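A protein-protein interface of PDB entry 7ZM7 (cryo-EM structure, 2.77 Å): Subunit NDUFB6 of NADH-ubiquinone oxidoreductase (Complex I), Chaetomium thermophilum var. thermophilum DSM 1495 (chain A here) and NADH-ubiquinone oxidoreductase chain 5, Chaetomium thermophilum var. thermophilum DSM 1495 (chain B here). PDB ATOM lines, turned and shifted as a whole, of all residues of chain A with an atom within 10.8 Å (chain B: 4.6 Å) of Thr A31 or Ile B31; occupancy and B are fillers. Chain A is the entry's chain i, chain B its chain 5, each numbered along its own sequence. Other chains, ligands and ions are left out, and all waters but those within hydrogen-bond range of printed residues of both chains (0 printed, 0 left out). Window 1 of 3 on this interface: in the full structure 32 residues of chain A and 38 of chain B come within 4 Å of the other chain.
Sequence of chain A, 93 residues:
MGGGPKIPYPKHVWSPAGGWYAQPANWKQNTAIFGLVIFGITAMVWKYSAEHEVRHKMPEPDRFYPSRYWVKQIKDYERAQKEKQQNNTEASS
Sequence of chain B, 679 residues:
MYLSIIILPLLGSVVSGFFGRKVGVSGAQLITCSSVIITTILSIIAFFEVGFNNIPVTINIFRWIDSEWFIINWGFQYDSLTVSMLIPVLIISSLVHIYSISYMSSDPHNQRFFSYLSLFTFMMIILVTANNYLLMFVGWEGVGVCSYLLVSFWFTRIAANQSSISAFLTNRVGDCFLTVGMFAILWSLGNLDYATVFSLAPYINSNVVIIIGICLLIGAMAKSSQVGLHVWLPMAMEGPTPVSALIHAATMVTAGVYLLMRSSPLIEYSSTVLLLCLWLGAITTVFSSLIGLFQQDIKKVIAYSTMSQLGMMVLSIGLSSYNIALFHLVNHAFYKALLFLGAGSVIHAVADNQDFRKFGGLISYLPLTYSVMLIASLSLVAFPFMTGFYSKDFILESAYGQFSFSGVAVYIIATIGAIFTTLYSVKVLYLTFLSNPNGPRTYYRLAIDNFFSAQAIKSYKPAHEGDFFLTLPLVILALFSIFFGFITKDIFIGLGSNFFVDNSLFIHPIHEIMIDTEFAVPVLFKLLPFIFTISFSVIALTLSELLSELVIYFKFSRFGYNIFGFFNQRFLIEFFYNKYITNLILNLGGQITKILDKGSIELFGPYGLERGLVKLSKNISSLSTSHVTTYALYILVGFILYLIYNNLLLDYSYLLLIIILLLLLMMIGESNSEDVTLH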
ATOM      1  N   ALA A  22      16.583 -23.855  32.593  1.00  0.00           N
ATOM      2  CA  ALA A  22      15.901 -22.624  32.137  1.00  0.00           C
ATOM      3  C   ALA A  22      14.388 -22.605  32.281  1.00  0.00           C
ATOM      4  O   ALA A  22      13.709 -23.351  31.564  1.00  0.00           O
ATOM      5  CB  ALA A  22      16.291 -22.345  30.713  1.00  0.00           C
ATOM      6  N   GLN A  23      13.890 -21.761  33.179  1.00  0.00           N
ATOM      7  CA  GLN A  23      12.434 -21.536  33.262  1.00  0.00           C
ATOM      8  C   GLN A  23      12.288 -20.023  33.301  1.00  0.00           C
ATOM      9  O   GLN A  23      12.874 -19.420  34.208  1.00  0.00           O
ATOM     10  CB  GLN A  23      11.867 -22.159  34.532  1.00  0.00           C
ATOM     11  CG  GLN A  23      10.411 -21.810  34.788  1.00  0.00           C
ATOM     12  CD  GLN A  23       9.669 -23.036  35.250  1.00  0.00           C
ATOM     13  OE1 GLN A  23       9.935 -24.141  34.790  1.00  0.00           O
ATOM     14  NE2 GLN A  23       8.745 -22.852  36.177  1.00  0.00           N
ATOM     15  N   PRO A  24      11.572 -19.368  32.367  1.00  0.00           N
ATOM     16  CA  PRO A  24      11.366 -17.934  32.475  1.00  0.00           C
ATOM     17  C   PRO A  24      10.343 -17.612  33.571  1.00  0.00           C
ATOM     18  O   PRO A  24       9.707 -18.515  34.046  1.00  0.00           O
ATOM     19  CB  PRO A  24      10.835 -17.544  31.087  1.00  0.00           C
ATOM     20  CG  PRO A  24      10.199 -18.805  30.555  1.00  0.00           C
ATOM     21  CD  PRO A  24      10.996 -19.943  31.156  1.00  0.00           C
ATOM     22  N   ALA A  25      10.245 -16.348  33.965  1.00  0.00           N
ATOM     23  CA  ALA A  25       9.227 -15.916  34.938  1.00  0.00           C
ATOM     24  C   ALA A  25       7.876 -15.936  34.242  1.00  0.00           C
ATOM     25  O   ALA A  25       6.895 -16.368  34.870  1.00  0.00           O
ATOM     26  CB  ALA A  25       9.563 -14.541  35.426  1.00  0.00           C
ATOM     27  N   ASN A  26       7.837 -15.497  32.984  1.00  0.00           N
ATOM     28  CA  ASN A  26       6.556 -15.341  32.321  1.00  0.00           C
ATOM     29  C   ASN A  26       6.064 -16.634  31.704  1.00  0.00           C
ATOM     30  O   ASN A  26       5.196 -16.604  30.826  1.00  0.00           O
ATOM     31  CB  ASN A  26       6.639 -14.243  31.262  1.00  0.00           C
ATOM     32  CG  ASN A  26       7.676 -14.529  30.199  1.00  0.00           C
ATOM     33  OD1 ASN A  26       8.854 -14.605  30.484  1.00  0.00           O
ATOM     34  ND2 ASN A  26       7.237 -14.650  28.960  1.00  0.00           N
ATOM     35  N   TRP A  27       6.571 -17.768  32.179  1.00  0.00           N
ATOM     36  CA  TRP A  27       6.360 -19.041  31.506  1.00  0.00           C
ATOM     37  C   TRP A  27       4.899 -19.453  31.474  1.00  0.00           C
ATOM     38  O   TRP A  27       4.475 -20.134  30.537  1.00  0.00           O
ATOM     39  CB  TRP A  27       7.206 -20.108  32.179  1.00  0.00           C
ATOM     40  CG  TRP A  27       6.787 -20.453  33.550  1.00  0.00           C
ATOM     41  CD1 TRP A  27       7.248 -19.908  34.695  1.00  0.00           C
ATOM     42  CD2 TRP A  27       5.829 -21.435  33.932  1.00  0.00           C
ATOM     43  NE1 TRP A  27       6.644 -20.484  35.772  1.00  0.00           N
ATOM     44  CE2 TRP A  27       5.759 -21.423  35.327  1.00  0.00           C
ATOM     45  CE3 TRP A  27       5.025 -22.328  33.227  1.00  0.00           C
ATOM     46  CZ2 TRP A  27       4.936 -22.273  36.029  1.00  0.00           C
ATOM     47  CZ3 TRP A  27       4.203 -23.143  33.919  1.00  0.00           C
ATOM     48  CH2 TRP A  27       4.159 -23.118  35.307  1.00  0.00           C
ATOM     49  N   LYS A  28       4.119 -19.082  32.487  1.00  0.00           N
ATOM     50  CA  LYS A  28       2.708 -19.429  32.470  1.00  0.00           C
ATOM     51  C   LYS A  28       1.985 -18.712  31.344  1.00  0.00           C
ATOM     52  O   LYS A  28       1.063 -19.265  30.736  1.00  0.00           O
ATOM     53  CB  LYS A  28       2.071 -19.109  33.812  1.00  0.00           C
ATOM     54  CG  LYS A  28       2.619 -19.920  34.951  1.00  0.00           C
ATOM     55  CD  LYS A  28       1.877 -19.619  36.232  1.00  0.00           C
ATOM     56  CE  LYS A  28       2.434 -20.409  37.400  1.00  0.00           C
ATOM     57  NZ  LYS A  28       3.742 -19.865  37.855  1.00  0.00           N
ATOM     58  N   GLN A  29       2.382 -17.480  31.050  1.00  0.00           N
ATOM     59  CA  GLN A  29       1.774 -16.757  29.943  1.00  0.00           C
ATOM     60  C   GLN A  29       2.224 -17.324  28.608  1.00  0.00           C
ATOM     61  O   GLN A  29       1.411 -17.525  27.703  1.00  0.00           O
ATOM     62  CB  GLN A  29       2.095 -15.272  30.060  1.00  0.00           C
ATOM     63  CG  GLN A  29       1.440 -14.620  31.268  1.00  0.00           C
ATOM     64  CD  GLN A  29       2.207 -14.845  32.554  1.00  0.00           C
ATOM     65  OE1 GLN A  29       3.380 -15.208  32.537  1.00  0.00           O
ATOM     66  NE2 GLN A  29       1.538 -14.646  33.681  1.00  0.00           N
ATOM     67  N   ASN A  30       3.513 -17.617  28.475  1.00  0.00           N
ATOM     68  CA  ASN A  30       3.993 -18.279  27.271  1.00  0.00           C
ATOM     69  C   ASN A  30       3.348 -19.654  27.101  1.00  0.00           C
ATOM     70  O   ASN A  30       2.923 -20.015  26.000  1.00  0.00           O
ATOM     71  CB  ASN A  30       5.512 -18.382  27.320  1.00  0.00           C
ATOM     72  CG  ASN A  30       6.192 -17.067  27.002  1.00  0.00           C
ATOM     73  OD1 ASN A  30       7.269 -16.763  27.512  1.00  0.00           O
ATOM     74  ND2 ASN A  30       5.560 -16.272  26.155  1.00  0.00           N
ATOM     75  N   THR A  31       3.252 -20.428  28.183  1.00  0.00           N
ATOM     76  CA  THR A  31       2.627 -21.746  28.098  1.00  0.00           C
ATOM     77  C   THR A  31       1.175 -21.644  27.673  1.00  0.00           C
ATOM     78  O   THR A  31       0.719 -22.401  26.808  1.00  0.00           O
ATOM     79  CB  THR A  31       2.723 -22.468  29.435  1.00  0.00           C
ATOM     80  OG1 THR A  31       4.095 -22.546  29.843  1.00  0.00           O
ATOM     81  CG2 THR A  31       2.126 -23.859  29.339  1.00  0.00           C
ATOM     82  N   ALA A  32       0.432 -20.707  28.256  1.00  0.00           N
ATOM     83  CA  ALA A  32      -0.965 -20.543  27.885  1.00  0.00           C
ATOM     84  C   ALA A  32      -1.108 -20.217  26.409  1.00  0.00           C
ATOM     85  O   ALA A  32      -1.952 -20.799  25.721  1.00  0.00           O
ATOM     86  CB  ALA A  32      -1.603 -19.450  28.733  1.00  0.00           C
ATOM     87  N   ILE A  33      -0.287 -19.300  25.899  1.00  0.00           N
ATOM     88  CA  ILE A  33      -0.366 -18.926  24.489  1.00  0.00           C
ATOM     89  C   ILE A  33      -0.100 -20.129  23.599  1.00  0.00           C
ATOM     90  O   ILE A  33      -0.801 -20.356  22.608  1.00  0.00           O
ATOM     91  CB  ILE A  33       0.612 -17.778  24.187  1.00  0.00           C
ATOM     92  CG1 ILE A  33       0.288 -16.559  25.046  1.00  0.00           C
ATOM     93  CG2 ILE A  33       0.586 -17.420  22.721  1.00  0.00           C
ATOM     94  CD1 ILE A  33      -1.084 -15.999  24.812  1.00  0.00           C
ATOM     95  N   PHE A  34       0.909 -20.929  23.942  1.00  0.00           N
ATOM     96  CA  PHE A  34       1.192 -22.116  23.150  1.00  0.00           C
ATOM     97  C   PHE A  34       0.052 -23.111  23.206  1.00  0.00           C
ATOM     98  O   PHE A  34      -0.152 -23.865  22.253  1.00  0.00           O
ATOM     99  CB  PHE A  34       2.484 -22.771  23.619  1.00  0.00           C
ATOM    100  CG  PHE A  34       3.682 -22.272  22.906  1.00  0.00           C
ATOM    101  CD1 PHE A  34       3.780 -22.398  21.541  1.00  0.00           C
ATOM    102  CD2 PHE A  34       4.701 -21.654  23.590  1.00  0.00           C
ATOM    103  CE1 PHE A  34       4.883 -21.926  20.870  1.00  0.00           C
ATOM    104  CE2 PHE A  34       5.806 -21.177  22.927  1.00  0.00           C
ATOM    105  CZ  PHE A  34       5.894 -21.306  21.567  1.00  0.00           C
ATOM    106  N   GLY A  35      -0.692 -23.137  24.307  1.00  0.00           N
ATOM    107  CA  GLY A  35      -1.815 -24.050  24.399  1.00  0.00           C
ATOM    108  C   GLY A  35      -2.899 -23.732  23.393  1.00  0.00           C
ATOM    109  O   GLY A  35      -3.477 -24.630  22.783  1.00  0.00           O
ATOM    110  N   LEU A  36      -3.186 -22.445  23.199  1.00  0.00           N
ATOM    111  CA  LEU A  36      -4.220 -22.060  22.246  1.00  0.00           C
ATOM    112  C   LEU A  36      -3.777 -22.311  20.814  1.00  0.00           C
ATOM    113  O   LEU A  36      -4.559 -22.807  19.997  1.00  0.00           O
ATOM    114  CB  LEU A  36      -4.607 -20.596  22.443  1.00  0.00           C
ATOM    115  CG  LEU A  36      -5.663 -20.329  23.514  1.00  0.00           C
ATOM    116  CD1 LEU A  36      -5.111 -20.553  24.907  1.00  0.00           C
ATOM    117  CD2 LEU A  36      -6.194 -18.917  23.370  1.00  0.00           C
ATOM    118  N   VAL A  37      -2.528 -21.996  20.489  1.00  0.00           N
ATOM    119  CA  VAL A  37      -2.052 -22.229  19.135  1.00  0.00           C
ATOM    120  C   VAL A  37      -2.043 -23.722  18.823  1.00  0.00           C
ATOM    121  O   VAL A  37      -2.333 -24.124  17.693  1.00  0.00           O
ATOM    122  CB  VAL A  37      -0.676 -21.572  18.922  1.00  0.00           C
ATOM    123  CG1 VAL A  37       0.415 -22.322  19.639  1.00  0.00           C
ATOM    124  CG2 VAL A  37      -0.364 -21.462  17.438  1.00  0.00           C
ATOM    125  N   ILE A  38      -1.737 -24.570  19.812  1.00  0.00           N
ATOM    126  CA  ILE A  38      -1.938 -26.009  19.640  1.00  0.00           C
ATOM    127  C   ILE A  38      -3.412 -26.315  19.438  1.00  0.00           C
ATOM    128  O   ILE A  38      -3.797 -26.996  18.482  1.00  0.00           O
ATOM    129  CB  ILE A  38      -1.373 -26.798  20.839  1.00  0.00           C
ATOM    130  CG1 ILE A  38       0.135 -26.640  20.961  1.00  0.00           C
ATOM    131  CG2 ILE A  38      -1.743 -28.258  20.772  1.00  0.00           C
ATOM    132  CD1 ILE A  38       0.672 -27.183  22.251  1.00  0.00           C
ATOM    133  N   PHE A  39      -4.259 -25.803  20.335  1.00  0.00           N
ATOM    134  CA  PHE A  39      -5.678 -26.136  20.311  1.00  0.00           C
ATOM    135  C   PHE A  39      -6.336 -25.655  19.027  1.00  0.00           C
ATOM    136  O   PHE A  39      -7.246 -26.302  18.505  1.00  0.00           O
ATOM    137  CB  PHE A  39      -6.360 -25.545  21.546  1.00  0.00           C
ATOM    138  CG  PHE A  39      -7.860 -25.489  21.459  1.00  0.00           C
ATOM    139  CD1 PHE A  39      -8.629 -26.558  21.883  1.00  0.00           C
ATOM    140  CD2 PHE A  39      -8.503 -24.353  20.994  1.00  0.00           C
ATOM    141  CE1 PHE A  39     -10.005 -26.508  21.818  1.00  0.00           C
ATOM    142  CE2 PHE A  39      -9.878 -24.298  20.925  1.00  0.00           C
ATOM    143  CZ  PHE A  39     -10.631 -25.376  21.339  1.00  0.00           C
ATOM    144  N   GLY B  12       3.016 -31.191  20.634  1.00  0.00           N
ATOM    145  CA  GLY B  12       3.647 -30.963  21.918  1.00  0.00           C
ATOM    146  C   GLY B  12       5.155 -31.040  21.852  1.00  0.00           C
ATOM    147  O   GLY B  12       5.850 -30.325  22.570  1.00  0.00           O
ATOM    148  N   VAL B  15       6.746 -27.692  20.550  1.00  0.00           N
ATOM    149  CA  VAL B  15       6.807 -26.669  21.582  1.00  0.00           C
ATOM    150  C   VAL B  15       7.941 -26.957  22.551  1.00  0.00           C
ATOM    151  O   VAL B  15       8.722 -26.067  22.899  1.00  0.00           O
ATOM    152  CB  VAL B  15       5.455 -26.575  22.309  1.00  0.00           C
ATOM    153  CG1 VAL B  15       5.527 -25.548  23.415  1.00  0.00           C
ATOM    154  CG2 VAL B  15       4.340 -26.265  21.326  1.00  0.00           C
ATOM    155  N   VAL B  23       8.569 -21.546  27.109  1.00  0.00           N
ATOM    156  CA  VAL B  23       7.677 -22.142  28.094  1.00  0.00           C
ATOM    157  C   VAL B  23       8.385 -22.576  29.367  1.00  0.00           C
ATOM    158  O   VAL B  23       7.724 -22.736  30.400  1.00  0.00           O
ATOM    159  CB  VAL B  23       6.934 -23.348  27.494  1.00  0.00           C
ATOM    160  CG1 VAL B  23       6.031 -22.903  26.414  1.00  0.00           C
ATOM    161  CG2 VAL B  23       7.929 -24.351  26.964  1.00  0.00           C
ATOM    162  N   GLY B  27       6.604 -25.367  31.856  1.00  0.00           N
ATOM    163  CA  GLY B  27       5.727 -25.189  30.719  1.00  0.00           C
ATOM    164  C   GLY B  27       5.834 -26.327  29.734  1.00  0.00           C
ATOM    165  O   GLY B  27       4.826 -26.812  29.221  1.00  0.00           O
ATOM    166  N   ALA B  28       7.060 -26.772  29.462  1.00  0.00           N
ATOM    167  CA  ALA B  28       7.247 -27.928  28.598  1.00  0.00           C
ATOM    168  C   ALA B  28       6.616 -29.175  29.197  1.00  0.00           C
ATOM    169  O   ALA B  28       5.926 -29.921  28.501  1.00  0.00           O
ATOM    170  CB  ALA B  28       8.732 -28.152  28.344  1.00  0.00           C
ATOM    171  N   GLN B  29       6.816 -29.402  30.492  1.00  0.00           N
ATOM    172  CA  GLN B  29       6.315 -30.626  31.105  1.00  0.00           C
ATOM    173  C   GLN B  29       4.806 -30.701  31.011  1.00  0.00           C
ATOM    174  O   GLN B  29       4.253 -31.754  30.692  1.00  0.00           O
ATOM    175  CB  GLN B  29       6.767 -30.720  32.560  1.00  0.00           C
ATOM    176  CG  GLN B  29       8.146 -31.295  32.741  1.00  0.00           C
ATOM    177  CD  GLN B  29       8.676 -31.086  34.139  1.00  0.00           C
ATOM    178  OE1 GLN B  29       8.169 -30.254  34.883  1.00  0.00           O
ATOM    179  NE2 GLN B  29       9.695 -31.844  34.510  1.00  0.00           N
ATOM    180  N   LEU B  30       4.119 -29.596  31.265  1.00  0.00           N
ATOM    181  CA  LEU B  30       2.665 -29.609  31.191  1.00  0.00           C
ATOM    182  C   LEU B  30       2.188 -29.863  29.765  1.00  0.00           C
ATOM    183  O   LEU B  30       1.323 -30.708  29.534  1.00  0.00           O
ATOM    184  CB  LEU B  30       2.112 -28.299  31.741  1.00  0.00           C
ATOM    185  CG  LEU B  30       0.612 -28.135  31.937  1.00  0.00           C
ATOM    186  CD1 LEU B  30       0.394 -27.135  33.033  1.00  0.00           C
ATOM    187  CD2 LEU B  30      -0.079 -27.657  30.683  1.00  0.00           C
ATOM    188  N   ILE B  31       2.746 -29.150  28.791  1.00  0.00           N
ATOM    189  CA  ILE B  31       2.272 -29.289  27.418  1.00  0.00           C
ATOM    190  C   ILE B  31       2.587 -30.673  26.869  1.00  0.00           C
ATOM    191  O   ILE B  31       1.724 -31.343  26.294  1.00  0.00           O
ATOM    192  CB  ILE B  31       2.855 -28.177  26.532  1.00  0.00           C
ATOM    193  CG1 ILE B  31       2.351 -26.812  27.004  1.00  0.00           C
ATOM    194  CG2 ILE B  31       2.582 -28.450  25.081  1.00  0.00           C
ATOM    195  CD1 ILE B  31       3.049 -25.648  26.375  1.00  0.00           C
ATOM    196  N   THR B  32       3.821 -31.124  27.041  1.00  0.00           N
ATOM    197  CA  THR B  32       4.177 -32.472  26.621  1.00  0.00           C
ATOM    198  C   THR B  32       3.297 -33.516  27.293  1.00  0.00           C
ATOM    199  O   THR B  32       2.740 -34.396  26.629  1.00  0.00           O
ATOM    200  CB  THR B  32       5.651 -32.724  26.919  1.00  0.00           C
ATOM    201  OG1 THR B  32       6.450 -31.992  25.991  1.00  0.00           O
ATOM    202  CG2 THR B  32       5.970 -34.157  26.839  1.00  0.00           C
ATOM    203  N   CYS B  33       3.153 -33.440  28.611  1.00  0.00           N
ATOM    204  CA  CYS B  33       2.371 -34.454  29.300  1.00  0.00           C
ATOM    205  C   CYS B  33       0.903 -34.360  28.923  1.00  0.00           C
ATOM    206  O   CYS B  33       0.293 -35.350  28.521  1.00  0.00           O
ATOM    207  CB  CYS B  33       2.552 -34.334  30.811  1.00  0.00           C
ATOM    208  SG  CYS B  33       4.159 -34.902  31.372  1.00  0.00           S
ATOM    209  N   SER B  34       0.329 -33.164  29.009  1.00  0.00           N
ATOM    210  CA  SER B  34      -1.102 -33.019  28.783  1.00  0.00           C
ATOM    211  C   SER B  34      -1.482 -33.375  27.354  1.00  0.00           C
ATOM    212  O   SER B  34      -2.540 -33.961  27.118  1.00  0.00           O
ATOM    213  CB  SER B  34      -1.548 -31.599  29.125  1.00  0.00           C
ATOM    214  OG  SER B  34      -0.871 -30.644  28.333  1.00  0.00           O
ATOM    215  N   SER B  35      -0.647 -33.006  26.385  1.00  0.00           N
ATOM    216  CA  SER B  35      -0.965 -33.303  24.994  1.00  0.00           C
ATOM    217  C   SER B  35      -0.994 -34.802  24.752  1.00  0.00           C
ATOM    218  O   SER B  35      -1.866 -35.308  24.039  1.00  0.00           O
ATOM    219  CB  SER B  35       0.046 -32.630  24.069  1.00  0.00           C
ATOM    220  OG  SER B  35       0.060 -31.226  24.279  1.00  0.00           O
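The indole nitrogen (NE1) of Trp A27 sits close to the side-chain amide nitrogen (NE2) of Gln A23, 3.2 Å away. The backbone carbonyl oxygen of Ile B31 sits at hydrogen-bond distance from the side-chain hydroxyl of Ser B34, at 3.4 Å. O of Ile B31 lies within hydrogen-bond range of OG of Ser B35 (2.6 Å). The side-chain hydroxyl (OG1) of Thr A31 sits at hydrogen-bond distance from the backbone carbonyl oxygen (O) of Trp A27.
Among the printed residues, merely in contact across the chains: Trp A27 with Val B23 (3.2 Å), Thr A31 with Gly B27 (3.2 Å), Phe A34 with Val B23 (3.4 Å), Thr A31 with Ile B31 (3.6 Å), Ile A38 with Ile B31 (3.6 Å), Thr A31 with Val B23 (3.7 Å), Trp A27 with Gly B27 (3.7 Å), Phe A34 with Val B15 (3.8 Å) and Ile A38 with Val B15 (3.9 Å).
Printed residues of chain B within 4 Å of Trp A27: Val B23 and Gly B27. Of chain B, only Val B23 (3.7 Å), Gly B27 (3.2 Å) and Ile B31 (3.6 Å) come within 4 Å of Thr A31. Printed residues of chain B within 4 Å of Phe A34: Val B15 (3.8 Å) and Val B23 (3.4 Å). Of the printed residues of chain B, Ile A38 touches Val B15 (3.9 Å) and Ile B31 (3.6 Å). Gly B12 touches none of the printed residues of chain A. Of chain A, only Trp A27, Thr A31 and Phe A34 come within 4 Å of Val B23. Gly B27 touches just these residues of chain A: Trp A27 and Thr A31. Ala B28 touches none of the printed residues of chain A. No residue of chain A comes within 4 Å of Leu B30. Ile B31 touches just these residues of chain A: Thr A31 (3.6 Å) and Ile A38 (3.6 Å). No residue of chain A comes within 4 Å of Thr B32. No residue of chain A comes within 4 Å of Cys B33. No residue of chain A comes within 4 Å of Ser B34. No residue of chain A comes within 4 Å of Ser B35. The nearest residue of chain A that does not touch Ile B31 is Phe A34 (4.02 Å). The nearest printed residue of chain B that does not touch Ile A38 is Ser B35 (4.6 Å).
Of the 18 printed residues of chain A, 4 touch a printed residue of chain B. Printed residues of chain A that touch a printed residue of chain B: Trp A27, Thr A31, Phe A34 and Ile A38. Hydrophobic or aromatic side chains of chain A within 4 Å of the printed part of chain B: Trp A27, Phe A34 and Ile A38. Of the 12 printed residues of chain B, 4 touch a printed residue of chain A. Hydrophobic or aromatic side chains of chain B that line the printed part of chain A: Val B15, Val B23 and Ile B31.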
